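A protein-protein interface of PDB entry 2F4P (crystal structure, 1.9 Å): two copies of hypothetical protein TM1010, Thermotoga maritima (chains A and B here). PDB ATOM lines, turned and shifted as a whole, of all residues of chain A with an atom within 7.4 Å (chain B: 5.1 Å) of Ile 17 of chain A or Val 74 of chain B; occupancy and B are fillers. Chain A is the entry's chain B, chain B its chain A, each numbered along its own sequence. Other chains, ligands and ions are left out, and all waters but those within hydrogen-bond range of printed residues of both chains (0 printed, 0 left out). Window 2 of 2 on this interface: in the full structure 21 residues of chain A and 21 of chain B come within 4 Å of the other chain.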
ATOM      1  N   ASP A  16     -23.717  -8.118  -0.659  1.00  0.00           N
ATOM      2  CA  ASP A  16     -24.820  -9.078  -0.395  1.00  0.00           C
ATOM      3  C   ASP A  16     -25.916  -8.509   0.529  1.00  0.00           C
ATOM      4  O   ASP A  16     -27.060  -8.381   0.107  1.00  0.00           O
ATOM      5  CB  ASP A  16     -24.276 -10.382   0.183  1.00  0.00           C
ATOM      6  CG  ASP A  16     -25.304 -11.479   0.183  1.00  0.00           C
ATOM      7  OD1 ASP A  16     -26.008 -11.628   1.217  1.00  0.00           O
ATOM      8  OD2 ASP A  16     -25.421 -12.171  -0.864  1.00  0.00           O
ATOM      9  N   ILE A  17     -25.575  -8.183   1.774  1.00  0.00           N
ATOM     10  CA  ILE A  17     -26.550  -7.610   2.737  1.00  0.00           C
ATOM     11  C   ILE A  17     -26.938  -6.177   2.364  1.00  0.00           C
ATOM     12  O   ILE A  17     -28.129  -5.821   2.401  1.00  0.00           O
ATOM     13  CB  ILE A  17     -26.023  -7.633   4.200  1.00  0.00           C
ATOM     14  CG1 ILE A  17     -25.804  -9.081   4.672  1.00  0.00           C
ATOM     15  CG2 ILE A  17     -27.021  -6.938   5.160  1.00  0.00           C
ATOM     16  CD1 ILE A  17     -24.919  -9.201   5.914  1.00  0.00           C
ATOM     17  N   PHE A  18     -25.940  -5.357   2.022  1.00  0.00           N
ATOM     18  CA  PHE A  18     -26.183  -3.955   1.665  1.00  0.00           C
ATOM     19  C   PHE A  18     -25.648  -3.626   0.289  1.00  0.00           C
ATOM     20  O   PHE A  18     -24.694  -4.265  -0.191  1.00  0.00           O
ATOM     21  CB  PHE A  18     -25.496  -3.010   2.645  1.00  0.00           C
ATOM     22  CG  PHE A  18     -25.806  -3.284   4.087  1.00  0.00           C
ATOM     23  CD1 PHE A  18     -26.974  -2.808   4.663  1.00  0.00           C
ATOM     24  CD2 PHE A  18     -24.906  -3.979   4.881  1.00  0.00           C
ATOM     25  CE1 PHE A  18     -27.255  -3.053   5.998  1.00  0.00           C
ATOM     26  CE2 PHE A  18     -25.182  -4.217   6.224  1.00  0.00           C
ATOM     27  CZ  PHE A  18     -26.350  -3.751   6.775  1.00  0.00           C
ATOM     28  N   GLU A  19     -26.218  -2.587  -0.322  1.00  0.00           N
ATOM     29  CA  GLU A  19     -25.620  -2.022  -1.540  1.00  0.00           C
ATOM     30  C   GLU A  19     -24.345  -1.296  -1.128  1.00  0.00           C
ATOM     31  O   GLU A  19     -24.181  -0.940   0.046  1.00  0.00           O
ATOM     32  CB  GLU A  19     -26.576  -1.052  -2.234  1.00  0.00           C
ATOM     33  N   LYS A  36     -20.963   2.997   3.403  1.00  0.00           N
ATOM     34  CA  LYS A  36     -22.398   3.237   3.519  1.00  0.00           C
ATOM     35  C   LYS A  36     -22.740   3.438   4.982  1.00  0.00           C
ATOM     36  O   LYS A  36     -22.513   2.553   5.826  1.00  0.00           O
ATOM     37  CB  LYS A  36     -23.180   2.054   2.952  1.00  0.00           C
ATOM     38  CG  LYS A  36     -24.672   2.227   3.001  1.00  0.00           C
ATOM     39  CD  LYS A  36     -25.377   0.905   2.903  1.00  0.00           C
ATOM     40  CE  LYS A  36     -26.878   1.089   3.068  1.00  0.00           C
ATOM     41  NZ  LYS A  36     -27.440   2.124   2.130  1.00  0.00           N
ATOM     42  N   LEU A  38     -25.054   3.380   8.041  1.00  0.00           N
ATOM     43  CA  LEU A  38     -26.269   2.654   8.434  1.00  0.00           C
ATOM     44  C   LEU A  38     -26.996   3.394   9.535  1.00  0.00           C
ATOM     45  O   LEU A  38     -28.231   3.520   9.501  1.00  0.00           O
ATOM     46  CB  LEU A  38     -25.899   1.260   8.908  1.00  0.00           C
ATOM     47  CG  LEU A  38     -25.190   0.424   7.839  1.00  0.00           C
ATOM     48  CD1 LEU A  38     -24.929  -0.979   8.366  1.00  0.00           C
ATOM     49  CD2 LEU A  38     -26.032   0.379   6.557  1.00  0.00           C
ATOM     50  N   ASP A  52     -21.219   0.381   7.004  1.00  0.00           N
ATOM     51  CA  ASP A  52     -20.809  -0.795   6.287  1.00  0.00           C
ATOM     52  C   ASP A  52     -19.735  -0.358   5.285  1.00  0.00           C
ATOM     53  O   ASP A  52     -19.841   0.689   4.640  1.00  0.00           O
ATOM     54  CB  ASP A  52     -21.999  -1.426   5.574  1.00  0.00           C
ATOM     55  CG  ASP A  52     -21.716  -2.829   5.072  1.00  0.00           C
ATOM     56  OD1 ASP A  52     -21.401  -3.722   5.893  1.00  0.00           O
ATOM     57  OD2 ASP A  52     -21.849  -3.062   3.852  1.00  0.00           O
ATOM     58  N   THR A  75     -18.396  -9.578   7.258  1.00  0.00           N
ATOM     59  CA  THR A  75     -19.502 -10.249   6.610  1.00  0.00           C
ATOM     60  C   THR A  75     -19.074 -11.013   5.342  1.00  0.00           C
ATOM     61  O   THR A  75     -19.759 -11.944   4.922  1.00  0.00           O
ATOM     62  CB  THR A  75     -20.628  -9.247   6.305  1.00  0.00           C
ATOM     63  OG1 THR A  75     -20.111  -8.174   5.525  1.00  0.00           O
ATOM     64  CG2 THR A  75     -21.199  -8.663   7.593  1.00  0.00           C
ATOM     65  N   ARG A  76     -17.954 -10.628   4.731  1.00  0.00           N
ATOM     66  CA  ARG A  76     -17.434 -11.356   3.577  1.00  0.00           C
ATOM     67  C   ARG A  76     -15.973 -11.066   3.335  1.00  0.00           C
ATOM     68  O   ARG A  76     -15.488  -9.990   3.657  1.00  0.00           O
ATOM     69  CB  ARG A  76     -18.201 -10.976   2.310  1.00  0.00           C
ATOM     70  CG  ARG A  76     -17.603 -11.561   1.012  1.00  0.00           C
ATOM     71  CD  ARG A  76     -18.593 -11.499  -0.147  1.00  0.00           C
ATOM     72  NE  ARG A  76     -19.027 -10.121  -0.374  1.00  0.00           N
ATOM     73  CZ  ARG A  76     -19.070  -9.498  -1.554  1.00  0.00           C
ATOM     74  NH1 ARG A  76     -18.735 -10.119  -2.685  1.00  0.00           N
ATOM     75  NH2 ARG A  76     -19.480  -8.228  -1.599  1.00  0.00           N
ATOM     76  N   LYS A  93     -14.843 -13.930   7.136  1.00  0.00           N
ATOM     77  CA  LYS A  93     -16.263 -13.856   7.444  1.00  0.00           C
ATOM     78  C   LYS A  93     -16.552 -14.402   8.829  1.00  0.00           C
ATOM     79  O   LYS A  93     -16.075 -15.474   9.191  1.00  0.00           O
ATOM     80  CB  LYS A  93     -17.051 -14.662   6.417  1.00  0.00           C
ATOM     81  CG  LYS A  93     -18.520 -14.576   6.633  1.00  0.00           C
ATOM     82  CD  LYS A  93     -19.291 -15.336   5.585  1.00  0.00           C
ATOM     83  CE  LYS A  93     -20.769 -15.269   5.912  1.00  0.00           C
ATOM     84  NZ  LYS A  93     -21.565 -16.100   4.978  1.00  0.00           N
ATOM     85  N   VAL A 116     -15.387  -7.021   3.326  1.00  0.00           N
ATOM     86  CA  VAL A 116     -16.624  -6.322   3.668  1.00  0.00           C
ATOM     87  C   VAL A 116     -16.921  -6.517   5.152  1.00  0.00           C
ATOM     88  O   VAL A 116     -16.946  -7.645   5.664  1.00  0.00           O
ATOM     89  CB  VAL A 116     -17.825  -6.841   2.838  1.00  0.00           C
ATOM     90  CG1 VAL A 116     -19.048  -5.970   3.050  1.00  0.00           C
ATOM     91  CG2 VAL A 116     -17.462  -6.923   1.347  1.00  0.00           C
ATOM     92  N   ILE A 118     -19.194  -4.694   8.706  1.00  0.00           N
ATOM     93  CA  ILE A 118     -19.897  -3.682   9.483  1.00  0.00           C
ATOM     94  C   ILE A 118     -18.951  -3.057  10.502  1.00  0.00           C
ATOM     95  O   ILE A 118     -18.073  -3.722  11.051  1.00  0.00           O
ATOM     96  CB  ILE A 118     -21.111  -4.316  10.208  1.00  0.00           C
ATOM     97  CG1 ILE A 118     -22.108  -4.824   9.166  1.00  0.00           C
ATOM     98  CG2 ILE A 118     -21.786  -3.287  11.124  1.00  0.00           C
ATOM     99  CD1 ILE A 118     -23.125  -5.832   9.700  1.00  0.00           C
ATOM    100  N   LEU B  72     -31.104  -2.692  15.346  1.00  0.00           N
ATOM    101  CA  LEU B  72     -31.178  -4.006  14.699  1.00  0.00           C
ATOM    102  C   LEU B  72     -30.715  -3.884  13.256  1.00  0.00           C
ATOM    103  O   LEU B  72     -31.039  -2.907  12.569  1.00  0.00           O
ATOM    104  CB  LEU B  72     -32.602  -4.552  14.675  1.00  0.00           C
ATOM    105  CG  LEU B  72     -33.424  -4.476  15.961  1.00  0.00           C
ATOM    106  CD1 LEU B  72     -34.758  -5.161  15.733  1.00  0.00           C
ATOM    107  CD2 LEU B  72     -32.689  -5.110  17.114  1.00  0.00           C
ATOM    108  N   ILE B  73     -29.958  -4.886  12.813  1.00  0.00           N
ATOM    109  CA  ILE B  73     -29.475  -4.968  11.448  1.00  0.00           C
ATOM    110  C   ILE B  73     -29.840  -6.346  10.937  1.00  0.00           C
ATOM    111  O   ILE B  73     -29.288  -7.339  11.405  1.00  0.00           O
ATOM    112  CB  ILE B  73     -27.953  -4.779  11.375  1.00  0.00           C
ATOM    113  CG1 ILE B  73     -27.540  -3.444  12.007  1.00  0.00           C
ATOM    114  CG2 ILE B  73     -27.504  -4.864   9.944  1.00  0.00           C
ATOM    115  CD1 ILE B  73     -26.031  -3.285  12.163  1.00  0.00           C
ATOM    116  N   VAL B  74     -30.794  -6.399  10.015  1.00  0.00           N
ATOM    117  CA  VAL B  74     -31.343  -7.660   9.523  1.00  0.00           C
ATOM    118  C   VAL B  74     -30.445  -8.236   8.453  1.00  0.00           C
ATOM    119  O   VAL B  74     -30.130  -7.567   7.470  1.00  0.00           O
ATOM    120  CB  VAL B  74     -32.771  -7.458   8.977  1.00  0.00           C
ATOM    121  CG1 VAL B  74     -33.368  -8.796   8.533  1.00  0.00           C
ATOM    122  CG2 VAL B  74     -33.630  -6.764  10.033  1.00  0.00           C
ATOM    123  N   THR B  75     -30.022  -9.476   8.651  1.00  0.00           N
ATOM    124  CA  THR B  75     -29.085 -10.119   7.734  1.00  0.00           C
ATOM    125  C   THR B  75     -29.723 -11.193   6.869  1.00  0.00           C
ATOM    126  O   THR B  75     -29.171 -11.535   5.830  1.00  0.00           O
ATOM    127  CB  THR B  75     -27.883 -10.734   8.481  1.00  0.00           C
ATOM    128  OG1 THR B  75     -28.327 -11.718   9.422  1.00  0.00           O
ATOM    129  CG2 THR B  75     -27.135  -9.679   9.230  1.00  0.00           C
ATOM    130  N   ARG B  76     -30.884 -11.708   7.269  1.00  0.00           N
ATOM    131  CA  ARG B  76     -31.525 -12.769   6.526  1.00  0.00           C
ATOM    132  C   ARG B  76     -32.982 -12.926   6.901  1.00  0.00           C
ATOM    133  O   ARG B  76     -33.362 -12.758   8.061  1.00  0.00           O
ATOM    134  CB  ARG B  76     -30.769 -14.071   6.785  1.00  0.00           C
ATOM    135  CG  ARG B  76     -31.428 -15.335   6.290  1.00  0.00           C
ATOM    136  CD  ARG B  76     -30.361 -16.347   5.983  1.00  0.00           C
ATOM    137  NE  ARG B  76     -30.764 -17.732   6.154  1.00  0.00           N
ATOM    138  CZ  ARG B  76     -30.702 -18.410   7.302  1.00  0.00           C
ATOM    139  NH1 ARG B  76     -30.308 -17.817   8.419  1.00  0.00           N
ATOM    140  NH2 ARG B  76     -31.059 -19.696   7.338  1.00  0.00           N
ATOM    141  N   GLY B  77     -33.804 -13.282   5.918  1.00  0.00           N
ATOM    142  CA  GLY B  77     -35.171 -13.724   6.208  1.00  0.00           C
ATOM    143  C   GLY B  77     -36.194 -12.609   6.253  1.00  0.00           C
ATOM    144  O   GLY B  77     -36.039 -11.600   5.578  1.00  0.00           O
ATOM    145  N   LEU B  91     -39.723  -6.483   8.316  1.00  0.00           N
ATOM    146  CA  LEU B  91     -38.277  -6.455   8.196  1.00  0.00           C
ATOM    147  C   LEU B  91     -37.804  -7.465   7.156  1.00  0.00           C
ATOM    148  O   LEU B  91     -38.300  -8.605   7.113  1.00  0.00           O
ATOM    149  CB  LEU B  91     -37.651  -6.820   9.540  1.00  0.00           C
ATOM    150  CG  LEU B  91     -38.061  -6.026  10.775  1.00  0.00           C
ATOM    151  CD1 LEU B  91     -37.379  -6.628  12.006  1.00  0.00           C
ATOM    152  CD2 LEU B  91     -37.740  -4.544  10.613  1.00  0.00           C
ATOM    153  N   LYS B  92     -36.832  -7.047   6.339  1.00  0.00           N
ATOM    154  CA  LYS B  92     -36.126  -7.927   5.402  1.00  0.00           C
ATOM    155  C   LYS B  92     -34.620  -7.657   5.448  1.00  0.00           C
ATOM    156  O   LYS B  92     -34.178  -6.673   6.060  1.00  0.00           O
ATOM    157  CB  LYS B  92     -36.626  -7.689   3.978  1.00  0.00           C
ATOM    158  CG  LYS B  92     -38.108  -8.035   3.768  1.00  0.00           C
ATOM    159  N   LYS B  93     -33.848  -8.504   4.772  1.00  0.00           N
ATOM    160  CA  LYS B  93     -32.390  -8.359   4.691  1.00  0.00           C
ATOM    161  C   LYS B  93     -31.994  -6.933   4.330  1.00  0.00           C
ATOM    162  O   LYS B  93     -32.507  -6.358   3.367  1.00  0.00           O
ATOM    163  CB  LYS B  93     -31.787  -9.337   3.662  1.00  0.00           C
ATOM    164  CG  LYS B  93     -30.258  -9.273   3.534  1.00  0.00           C
ATOM    165  CD  LYS B  93     -29.684 -10.395   2.649  1.00  0.00           C
ATOM    166  CE  LYS B  93     -29.578 -10.000   1.179  1.00  0.00           C
ATOM    167  N   GLY B  94     -31.077  -6.371   5.107  1.00  0.00           N
ATOM    168  CA  GLY B  94     -30.559  -5.020   4.860  1.00  0.00           C
ATOM    169  C   GLY B  94     -31.191  -3.925   5.695  1.00  0.00           C
ATOM    170  O   GLY B  94     -30.651  -2.801   5.790  1.00  0.00           O
ATOM    171  N   ASP B  95     -32.331  -4.225   6.308  1.00  0.00           N
ATOM    172  CA  ASP B  95     -33.065  -3.214   7.055  1.00  0.00           C
ATOM    173  C   ASP B  95     -32.327  -2.894   8.343  1.00  0.00           C
ATOM    174  O   ASP B  95     -31.686  -3.762   8.960  1.00  0.00           O
ATOM    175  CB  ASP B  95     -34.489  -3.686   7.381  1.00  0.00           C
ATOM    176  CG  ASP B  95     -35.412  -3.650   6.156  1.00  0.00           C
ATOM    177  OD1 ASP B  95     -34.999  -3.125   5.094  1.00  0.00           O
ATOM    178  OD2 ASP B  95     -36.538  -4.180   6.236  1.00  0.00           O
ATOM    179  N   LEU B 115     -36.117 -15.134  10.937  1.00  0.00           N
ATOM    180  CA  LEU B 115     -35.456 -13.820  10.930  1.00  0.00           C
ATOM    181  C   LEU B 115     -34.104 -13.967  11.609  1.00  0.00           C
ATOM    182  O   LEU B 115     -33.998 -14.595  12.660  1.00  0.00           O
ATOM    183  CB  LEU B 115     -36.280 -12.762  11.657  1.00  0.00           C
ATOM    184  CG  LEU B 115     -35.613 -11.388  11.847  1.00  0.00           C
ATOM    185  CD1 LEU B 115     -35.604 -10.601  10.557  1.00  0.00           C
ATOM    186  CD2 LEU B 115     -36.306 -10.625  12.958  1.00  0.00           C
ATOM    187  N   VAL B 116     -33.074 -13.427  10.965  1.00  0.00           N
ATOM    188  CA  VAL B 116     -31.740 -13.363  11.537  1.00  0.00           C
ATOM    189  C   VAL B 116     -31.309 -11.922  11.529  1.00  0.00           C
ATOM    190  O   VAL B 116     -31.422 -11.232  10.496  1.00  0.00           O
ATOM    191  CB  VAL B 116     -30.712 -14.177  10.732  1.00  0.00           C
ATOM    192  CG1 VAL B 116     -29.330 -14.190  11.452  1.00  0.00           C
ATOM    193  CG2 VAL B 116     -31.246 -15.595  10.477  1.00  0.00           C
ATOM    194  N   HIS B 117     -30.805 -11.465  12.670  1.00  0.00           N
ATOM    195  CA  HIS B 117     -30.320 -10.114  12.748  1.00  0.00           C
ATOM    196  C   HIS B 117     -29.193  -9.958  13.773  1.00  0.00           C
ATOM    197  O   HIS B 117     -29.071 -10.757  14.714  1.00  0.00           O
ATOM    198  CB  HIS B 117     -31.482  -9.134  13.023  1.00  0.00           C
ATOM    199  CG  HIS B 117     -31.952  -9.120  14.435  1.00  0.00           C
ATOM    200  ND1 HIS B 117     -31.295  -8.427  15.426  1.00  0.00           N
ATOM    201  CD2 HIS B 117     -33.031  -9.692  15.023  1.00  0.00           C
ATOM    202  CE1 HIS B 117     -31.924  -8.608  16.573  1.00  0.00           C
ATOM    203  NE2 HIS B 117     -32.991  -9.356  16.353  1.00  0.00           N
ATOM    204  N   ILE B 118     -28.371  -8.931  13.547  1.00  0.00           N
ATOM    205  CA  ILE B 118     -27.443  -8.429  14.533  1.00  0.00           C
ATOM    206  C   ILE B 118     -28.205  -7.433  15.393  1.00  0.00           C
ATOM    207  O   ILE B 118     -29.044  -6.666  14.894  1.00  0.00           O
ATOM    208  CB  ILE B 118     -26.215  -7.754  13.860  1.00  0.00           C
ATOM    209  CG1 ILE B 118     -25.386  -8.801  13.086  1.00  0.00           C
ATOM    210  CG2 ILE B 118     -25.321  -7.056  14.902  1.00  0.00           C
ATOM    211  CD1 ILE B 118     -24.576  -8.234  11.949  1.00  0.00           C
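The backbone NH (N) of Ile 118 of chain B is in hydrogen-bond range of the backbone carbonyl oxygen (O) of Ile 73 of chain B (2.8 Å). The backbone carbonyl oxygen (O) of Asp 95 of chain B lies within hydrogen-bond range of the backbone NH (N) of Val 74 of chain B (3.0 Å). The backbone carbonyl oxygen (O) of Val 74 of chain B lies within hydrogen-bond range of the backbone NH (N) of Gly 94 of chain B (2.8 Å).
Among the printed residues, pairs that only touch across the chains: Asp 16 of chain A with Lys 93 of chain B (3.2 Å), Ile 17 of chain A with Val 74 of chain B (3.9 Å), Ile 17 of chain A with Gly 94 of chain B (3.5 Å), Phe 18 of chain A with Ile 73 of chain B (3.6 Å), Phe 18 of chain A with Gly 94 of chain B (3.4 Å) and Ile 118 of chain A with Ile 118 of chain B (3.6 Å).
Of the printed residues of chain B, Ile 17 of chain A touches Val 74 (3.9 Å) and Gly 94 (3.5 Å). Of the printed residues of chain B, Ile 118 of chain A touches Ile 118. Of the printed residues of chain A, Gly 94 of chain B touches Ile 17 and Phe 18. Leu 38 of chain A touches none of the printed residues of chain B. Leu 91 of chain B touches none of the printed residues of chain A. The nearest printed residue of chain B that does not touch Ile 17 of chain A is Thr 75 of chain B (4.02 Å). The nearest residue of chain A that does not touch Val 74 of chain B is Phe 18 of chain A (5.4 Å). The nearest printed residue of chain A that does not touch Ile 73 of chain B is Ile 118 of chain A (4.4 Å).
Of the 15 printed residues of chain B, 5 touch a printed residue of chain A. Printed residues of chain B that touch a printed residue of chain A: Ile 73, Val 74, Lys 93, Gly 94 and Ile 118. Among the printed residues, 6 pairs touch across the chains. Among the printed residues, no Asp or Glu carboxylate lies within 4 Å of a Lys or Arg side-chain nitrogen of the other chain.
Ile 118 of chain A touches its own counterpart, Ile 118 of chain B.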
